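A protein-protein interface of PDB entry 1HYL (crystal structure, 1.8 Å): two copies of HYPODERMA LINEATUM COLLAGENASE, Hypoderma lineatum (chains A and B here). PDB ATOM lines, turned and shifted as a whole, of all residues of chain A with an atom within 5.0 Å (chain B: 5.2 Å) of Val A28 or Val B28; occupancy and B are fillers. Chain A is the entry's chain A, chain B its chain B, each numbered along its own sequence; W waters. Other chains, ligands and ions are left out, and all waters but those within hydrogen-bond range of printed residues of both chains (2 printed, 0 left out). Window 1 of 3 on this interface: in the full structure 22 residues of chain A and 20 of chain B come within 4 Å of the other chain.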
ATOM      1  N   LEU A  18      -1.739 -29.027   5.813  1.00  0.00           N
ATOM      2  CA  LEU A  18      -2.940 -28.919   5.015  1.00  0.00           C
ATOM      3  C   LEU A  18      -3.938 -28.074   5.747  1.00  0.00           C
ATOM      4  O   LEU A  18      -4.334 -28.417   6.862  1.00  0.00           O
ATOM      5  CB  LEU A  18      -3.526 -30.300   4.778  1.00  0.00           C
ATOM      6  CG  LEU A  18      -2.608 -31.409   4.196  1.00  0.00           C
ATOM      7  CD1 LEU A  18      -3.376 -32.716   4.137  1.00  0.00           C
ATOM      8  CD2 LEU A  18      -2.133 -31.016   2.796  1.00  0.00           C
ATOM      9  N   ASP A  19      -4.313 -26.951   5.155  1.00  0.00           N
ATOM     10  CA  ASP A  19      -5.372 -26.130   5.693  1.00  0.00           C
ATOM     11  C   ASP A  19      -6.636 -26.517   4.889  1.00  0.00           C
ATOM     12  O   ASP A  19      -6.770 -26.172   3.708  1.00  0.00           O
ATOM     13  CB  ASP A  19      -4.976 -24.667   5.497  1.00  0.00           C
ATOM     14  CG  ASP A  19      -6.025 -23.713   6.061  1.00  0.00           C
ATOM     15  OD1 ASP A  19      -6.851 -24.125   6.960  1.00  0.00           O
ATOM     16  OD2 ASP A  19      -6.087 -22.501   5.638  1.00  0.00           O
ATOM     17  N   ILE A  20      -7.532 -27.237   5.551  1.00  0.00           N
ATOM     18  CA  ILE A  20      -8.720 -27.846   4.901  1.00  0.00           C
ATOM     19  C   ILE A  20     -10.020 -27.111   5.179  1.00  0.00           C
ATOM     20  O   ILE A  20     -10.239 -26.808   6.349  1.00  0.00           O
ATOM     21  CB  ILE A  20      -8.855 -29.294   5.418  1.00  0.00           C
ATOM     22  CG1 ILE A  20      -7.610 -30.153   5.140  1.00  0.00           C
ATOM     23  CG2 ILE A  20     -10.024 -30.060   4.799  1.00  0.00           C
ATOM     24  CD1 ILE A  20      -7.450 -31.328   6.113  1.00  0.00           C
ATOM     25  N   LEU A  22     -14.107 -27.566   5.043  1.00  0.00           N
ATOM     26  CA  LEU A  22     -15.000 -28.669   4.861  1.00  0.00           C
ATOM     27  C   LEU A  22     -16.270 -28.228   4.214  1.00  0.00           C
ATOM     28  O   LEU A  22     -16.508 -27.021   4.102  1.00  0.00           O
ATOM     29  CB  LEU A  22     -15.347 -29.303   6.176  1.00  0.00           C
ATOM     30  CG  LEU A  22     -14.250 -29.816   7.082  1.00  0.00           C
ATOM     31  CD1 LEU A  22     -14.938 -30.432   8.250  1.00  0.00           C
ATOM     32  CD2 LEU A  22     -13.331 -30.808   6.397  1.00  0.00           C
ATOM     33  N   ARG A  26     -16.233 -25.464   8.205  1.00  0.00           N
ATOM     34  CA  ARG A  26     -15.155 -25.390   9.205  1.00  0.00           C
ATOM     35  C   ARG A  26     -13.781 -25.573   8.594  1.00  0.00           C
ATOM     36  O   ARG A  26     -13.643 -26.148   7.506  1.00  0.00           O
ATOM     37  CB  ARG A  26     -15.307 -26.446  10.283  1.00  0.00           C
ATOM     38  CG  ARG A  26     -16.548 -26.269  11.105  1.00  0.00           C
ATOM     39  CD  ARG A  26     -17.062 -27.665  11.150  1.00  0.00           C
ATOM     40  NE  ARG A  26     -17.038 -28.178  12.459  1.00  0.00           N
ATOM     41  CZ  ARG A  26     -17.497 -29.388  12.759  1.00  0.00           C
ATOM     42  NH1 ARG A  26     -18.003 -30.273  11.907  1.00  0.00           N
ATOM     43  NH2 ARG A  26     -17.447 -29.673  14.034  1.00  0.00           N
ATOM     44  N   ARG A  27     -12.792 -25.048   9.323  1.00  0.00           N
ATOM     45  CA  ARG A  27     -11.377 -25.034   8.950  1.00  0.00           C
ATOM     46  C   ARG A  27     -10.699 -26.050   9.836  1.00  0.00           C
ATOM     47  O   ARG A  27     -10.725 -25.896  11.067  1.00  0.00           O
ATOM     48  CB  ARG A  27     -10.664 -23.688   9.216  1.00  0.00           C
ATOM     49  CG  ARG A  27     -10.476 -22.840   8.003  1.00  0.00           C
ATOM     50  CD  ARG A  27      -9.054 -22.283   7.941  1.00  0.00           C
ATOM     51  NE  ARG A  27      -8.722 -21.148   8.782  1.00  0.00           N
ATOM     52  CZ  ARG A  27      -7.619 -20.401   8.580  1.00  0.00           C
ATOM     53  NH1 ARG A  27      -6.690 -20.755   7.692  1.00  0.00           N
ATOM     54  NH2 ARG A  27      -7.411 -19.325   9.359  1.00  0.00           N
ATOM     55  N   VAL A  28     -10.095 -27.052   9.186  1.00  0.00           N
ATOM     56  CA  VAL A  28      -9.431 -28.175   9.822  1.00  0.00           C
ATOM     57  C   VAL A  28      -7.954 -28.123   9.452  1.00  0.00           C
ATOM     58  O   VAL A  28      -7.623 -27.646   8.363  1.00  0.00           O
ATOM     59  CB  VAL A  28     -10.115 -29.458   9.332  1.00  0.00           C
ATOM     60  CG1 VAL A  28      -9.428 -30.716   9.760  1.00  0.00           C
ATOM     61  CG2 VAL A  28     -11.424 -29.521  10.026  1.00  0.00           C
ATOM     62  N   TRP A  29      -7.036 -28.487  10.350  1.00  0.00           N
ATOM     63  CA  TRP A  29      -5.634 -28.588  10.003  1.00  0.00           C
ATOM     64  C   TRP A  29      -5.279 -30.085   9.999  1.00  0.00           C
ATOM     65  O   TRP A  29      -5.719 -30.814  10.900  1.00  0.00           O
ATOM     66  CB  TRP A  29      -4.730 -27.908  11.012  1.00  0.00           C
ATOM     67  CG  TRP A  29      -3.255 -28.058  10.622  1.00  0.00           C
ATOM     68  CD1 TRP A  29      -2.462 -29.061  11.124  1.00  0.00           C
ATOM     69  CD2 TRP A  29      -2.585 -27.262   9.722  1.00  0.00           C
ATOM     70  NE1 TRP A  29      -1.294 -28.909  10.539  1.00  0.00           N
ATOM     71  CE2 TRP A  29      -1.324 -27.834   9.707  1.00  0.00           C
ATOM     72  CE3 TRP A  29      -2.849 -26.156   8.938  1.00  0.00           C
ATOM     73  CZ2 TRP A  29      -0.326 -27.284   8.905  1.00  0.00           C
ATOM     74  CZ3 TRP A  29      -1.844 -25.614   8.137  1.00  0.00           C
ATOM     75  CH2 TRP A  29      -0.580 -26.170   8.111  1.00  0.00           C
ATOM     76  N   CYS A  30      -4.502 -30.585   9.023  1.00  0.00           N
ATOM     77  CA  CYS A  30      -3.938 -31.942   9.087  1.00  0.00           C
ATOM     78  C   CYS A  30      -2.553 -31.888   8.492  1.00  0.00           C
ATOM     79  O   CYS A  30      -2.159 -30.861   7.933  1.00  0.00           O
ATOM     80  CB  CYS A  30      -4.730 -32.952   8.285  1.00  0.00           C
ATOM     81  SG  CYS A  30      -6.205 -33.573   9.135  1.00  0.00           S
ATOM     82  N   CYS A  46      -9.325 -36.756   7.384  1.00  0.00           N
ATOM     83  CA  CYS A  46      -8.993 -35.356   7.282  1.00  0.00           C
ATOM     84  C   CYS A  46      -9.798 -34.740   6.170  1.00  0.00           C
ATOM     85  O   CYS A  46     -10.420 -33.689   6.339  1.00  0.00           O
ATOM     86  CB  CYS A  46      -7.498 -35.121   6.939  1.00  0.00           C
ATOM     87  SG  CYS A  46      -6.426 -35.427   8.384  1.00  0.00           S
ATOM     88  N   LEU B  18     -11.624 -20.600  20.144  1.00  0.00           N
ATOM     89  CA  LEU B  18     -11.962 -21.963  20.536  1.00  0.00           C
ATOM     90  C   LEU B  18     -11.197 -22.976  19.735  1.00  0.00           C
ATOM     91  O   LEU B  18     -11.349 -23.046  18.518  1.00  0.00           O
ATOM     92  CB  LEU B  18     -13.448 -22.259  20.320  1.00  0.00           C
ATOM     93  CG  LEU B  18     -14.531 -21.317  20.813  1.00  0.00           C
ATOM     94  CD1 LEU B  18     -15.888 -21.890  20.506  1.00  0.00           C
ATOM     95  CD2 LEU B  18     -14.424 -21.162  22.303  1.00  0.00           C
ATOM     96  N   ASP B  19     -10.409 -23.798  20.391  1.00  0.00           N
ATOM     97  CA  ASP B  19      -9.680 -24.876  19.750  1.00  0.00           C
ATOM     98  C   ASP B  19     -10.526 -26.126  20.014  1.00  0.00           C
ATOM     99  O   ASP B  19     -10.546 -26.615  21.162  1.00  0.00           O
ATOM    100  CB  ASP B  19      -8.298 -24.976  20.403  1.00  0.00           C
ATOM    101  CG  ASP B  19      -7.339 -25.971  19.760  1.00  0.00           C
ATOM    102  OD1 ASP B  19      -7.556 -26.437  18.652  1.00  0.00           O
ATOM    103  OD2 ASP B  19      -6.316 -26.284  20.344  1.00  0.00           O
ATOM    104  N   ILE B  20     -11.235 -26.680  19.018  1.00  0.00           N
ATOM    105  CA  ILE B  20     -12.211 -27.737  19.213  1.00  0.00           C
ATOM    106  C   ILE B  20     -11.649 -29.094  18.816  1.00  0.00           C
ATOM    107  O   ILE B  20     -11.006 -29.195  17.772  1.00  0.00           O
ATOM    108  CB  ILE B  20     -13.442 -27.391  18.365  1.00  0.00           C
ATOM    109  CG1 ILE B  20     -13.961 -25.998  18.775  1.00  0.00           C
ATOM    110  CG2 ILE B  20     -14.551 -28.392  18.593  1.00  0.00           C
ATOM    111  CD1 ILE B  20     -14.820 -25.279  17.702  1.00  0.00           C
ATOM    112  N   LEU B  22     -12.955 -32.703  17.595  1.00  0.00           N
ATOM    113  CA  LEU B  22     -14.184 -33.372  17.224  1.00  0.00           C
ATOM    114  C   LEU B  22     -14.110 -34.840  17.552  1.00  0.00           C
ATOM    115  O   LEU B  22     -13.044 -35.375  17.851  1.00  0.00           O
ATOM    116  CB  LEU B  22     -14.480 -33.254  15.740  1.00  0.00           C
ATOM    117  CG  LEU B  22     -14.458 -31.890  15.114  1.00  0.00           C
ATOM    118  CD1 LEU B  22     -14.910 -32.009  13.676  1.00  0.00           C
ATOM    119  CD2 LEU B  22     -15.350 -30.939  15.927  1.00  0.00           C
ATOM    120  N   ARG B  26     -10.630 -34.646  14.506  1.00  0.00           N
ATOM    121  CA  ARG B  26     -10.027 -33.483  13.848  1.00  0.00           C
ATOM    122  C   ARG B  26     -10.007 -32.236  14.734  1.00  0.00           C
ATOM    123  O   ARG B  26     -10.806 -32.158  15.684  1.00  0.00           O
ATOM    124  CB  ARG B  26     -10.767 -33.189  12.589  1.00  0.00           C
ATOM    125  CG  ARG B  26     -10.461 -34.160  11.438  1.00  0.00           C
ATOM    126  CD  ARG B  26     -11.883 -34.225  11.020  1.00  0.00           C
ATOM    127  NE  ARG B  26     -12.083 -33.882   9.682  1.00  0.00           N
ATOM    128  CZ  ARG B  26     -13.280 -33.920   9.099  1.00  0.00           C
ATOM    129  NH1 ARG B  26     -14.429 -34.182   9.680  1.00  0.00           N
ATOM    130  NH2 ARG B  26     -13.273 -33.684   7.825  1.00  0.00           N
ATOM    131  N   ARG B  27      -9.047 -31.333  14.482  1.00  0.00           N
ATOM    132  CA  ARG B  27      -8.890 -30.105  15.218  1.00  0.00           C
ATOM    133  C   ARG B  27      -9.409 -28.910  14.384  1.00  0.00           C
ATOM    134  O   ARG B  27      -8.966 -28.613  13.269  1.00  0.00           O
ATOM    135  CB  ARG B  27      -7.402 -30.026  15.602  1.00  0.00           C
ATOM    136  CG  ARG B  27      -7.125 -28.737  16.304  1.00  0.00           C
ATOM    137  CD  ARG B  27      -6.082 -28.784  17.345  1.00  0.00           C
ATOM    138  NE  ARG B  27      -4.821 -28.342  16.841  1.00  0.00           N
ATOM    139  CZ  ARG B  27      -4.011 -27.495  17.493  1.00  0.00           C
ATOM    140  NH1 ARG B  27      -4.328 -26.839  18.607  1.00  0.00           N
ATOM    141  NH2 ARG B  27      -2.832 -27.269  16.924  1.00  0.00           N
ATOM    142  N   VAL B  28     -10.421 -28.236  14.944  1.00  0.00           N
ATOM    143  CA  VAL B  28     -11.207 -27.171  14.324  1.00  0.00           C
ATOM    144  C   VAL B  28     -11.006 -25.848  15.084  1.00  0.00           C
ATOM    145  O   VAL B  28     -10.781 -25.891  16.297  1.00  0.00           O
ATOM    146  CB  VAL B  28     -12.694 -27.644  14.350  1.00  0.00           C
ATOM    147  CG1 VAL B  28     -13.665 -26.582  13.910  1.00  0.00           C
ATOM    148  CG2 VAL B  28     -12.871 -28.746  13.333  1.00  0.00           C
ATOM    149  N   TRP B  29     -11.006 -24.673  14.425  1.00  0.00           N
ATOM    150  CA  TRP B  29     -10.987 -23.370  15.113  1.00  0.00           C
ATOM    151  C   TRP B  29     -12.320 -22.632  14.894  1.00  0.00           C
ATOM    152  O   TRP B  29     -12.891 -22.630  13.796  1.00  0.00           O
ATOM    153  CB  TRP B  29      -9.903 -22.454  14.591  1.00  0.00           C
ATOM    154  CG  TRP B  29      -9.812 -21.165  15.408  1.00  0.00           C
ATOM    155  CD1 TRP B  29     -10.433 -20.020  14.970  1.00  0.00           C
ATOM    156  CD2 TRP B  29      -9.165 -20.996  16.619  1.00  0.00           C
ATOM    157  NE1 TRP B  29     -10.199 -19.124  15.893  1.00  0.00           N
ATOM    158  CE2 TRP B  29      -9.442 -19.651  16.884  1.00  0.00           C
ATOM    159  CE3 TRP B  29      -8.403 -21.718  17.525  1.00  0.00           C
ATOM    160  CZ2 TRP B  29      -8.957 -19.053  18.026  1.00  0.00           C
ATOM    161  CZ3 TRP B  29      -7.927 -21.113  18.667  1.00  0.00           C
ATOM    162  CH2 TRP B  29      -8.201 -19.783  18.911  1.00  0.00           C
ATOM    163  N   CYS B  30     -12.844 -22.022  15.952  1.00  0.00           N
ATOM    164  CA  CYS B  30     -14.018 -21.184  15.857  1.00  0.00           C
ATOM    165  C   CYS B  30     -13.819 -20.077  16.879  1.00  0.00           C
ATOM    166  O   CYS B  30     -12.902 -20.139  17.730  1.00  0.00           O
ATOM    167  CB  CYS B  30     -15.300 -21.984  16.175  1.00  0.00           C
ATOM    168  SG  CYS B  30     -15.891 -22.986  14.782  1.00  0.00           S
ATOM    169  N   CYS B  46     -20.076 -25.514  14.931  1.00  0.00           N
ATOM    170  CA  CYS B  46     -18.658 -25.598  15.365  1.00  0.00           C
ATOM    171  C   CYS B  46     -18.476 -26.761  16.274  1.00  0.00           C
ATOM    172  O   CYS B  46     -17.565 -27.550  16.084  1.00  0.00           O
ATOM    173  CB  CYS B  46     -18.262 -24.328  16.121  1.00  0.00           C
ATOM    174  SG  CYS B  46     -17.892 -22.893  15.000  1.00  0.00           S
HETATM  175  O   HOH W   1     -14.013 -23.513  11.534  1.00  0.00           O
HETATM  176  O   HOH W   2      -7.396 -32.372  12.406  1.00  0.00           O
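The guanidinium group of Arg A26 is in hydrogen-bond range of the backbone carbonyl oxygen of Cys B46 (3.0 Å).
The backbone carbonyl oxygen (O) of Cys A46 is in hydrogen-bond range of the guanidinium group (NH2) of Arg B26, at 3.2 Å.
OD2 of Asp A19 is in salt-bridge range of NH1 of Arg A27, 2.8 Å away.
The backbone NH of Ile A20 sits at hydrogen-bond distance from the backbone carbonyl oxygen of Val A28 (2.8 Å).
SG of Cys A46 is disulfide-bonded to SG of Cys A30 (2.0 Å).
The side-chain carboxylate of Asp B19 lies within salt-bridge range of the guanidinium group of Arg B27, 2.7 Å away.
The backbone carbonyl oxygen (O) of Val B28 sits at hydrogen-bond distance from the backbone NH (N) of Ile B20 (2.9 Å).
SG of Cys B30 forms a disulfide with SG of Cys B46, at 2.0 Å.
CD2 of Leu A22 touches NH2 of Arg B26 (3.2 Å).
Leu B22 touches Arg A26.
Val B28 touches Arg A26 (CG1 to CB, 3.98 Å).
Arg A27 touches Arg B27 (O to O, 3.9 Å).
Arg A27 touches Val B28 (O to CA, 3.5 Å).
Arg A27 touches Trp B29 (O to N, 3.6 Å).
Val A28 touches Arg B26 (CG1 to CG, 3.97 Å).
Val A28 touches Arg B27.
Val A28 touches Val B28.
Arg B27 touches Trp A29.
Of the printed residues of chain B, Arg A26 touches Leu B22 (3.1 Å), Val B28 (3.98 Å) and Cys B46 (3.0 Å).
Of the printed residues of chain B, Arg A27 touches Arg B27 (3.9 Å), Val B28 (3.5 Å) and Trp B29 (3.6 Å).
Val A28 touches just these residues of chain B: Arg B26 (3.97 Å), Arg B27 (3.5 Å) and Val B28 (3.7 Å).
Of the printed residues of chain A, Leu B22 touches Arg A26 (3.1 Å).
Of the printed residues of chain A, Arg B27 touches Arg A27, Val A28 and Trp A29.
Of the printed residues of chain A, Val B28 touches Arg A26 (3.98 Å), Arg A27 (3.5 Å) and Val A28 (3.7 Å).
Printed residues of chain A within 4 Å of Trp B29: Arg A27.
Hydrophobic or aromatic side chains of chain A within 4 Å of the printed part of chain B: Leu A22 and Val A28.
Of the 10 printed residues of chain B, 6 touch a printed residue of chain A.
Among the printed residues, no Asp or Glu carboxylate lies within 4 Å of a Lys or Arg side-chain nitrogen of the other chain.
Leu A22 touches Arg B26, and with the chains exchanged Arg A26 touches Leu B22.
Arg A26 touches Cys B46, and with the chains exchanged Cys A46 touches Arg B26.
Arg A27 touches its own counterpart, Arg B27.
Arg A27 touches Trp B29, and with the chains exchanged Trp A29 touches Arg B27.
10 positions are printed for both chains.
Water W1 lies within hydrogen-bond range of O of Trp B29 (2.7 Å), N of Arg A27 (3.0 Å) and SG of Cys B30 (3.8 Å).
Water W2 lies within hydrogen-bond range of the backbone carbonyl oxygen of Trp A29 (2.7 Å), the backbone NH of Arg B27 (2.8 Å) and the side-chain sulfur of Cys A30 (3.7 Å).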
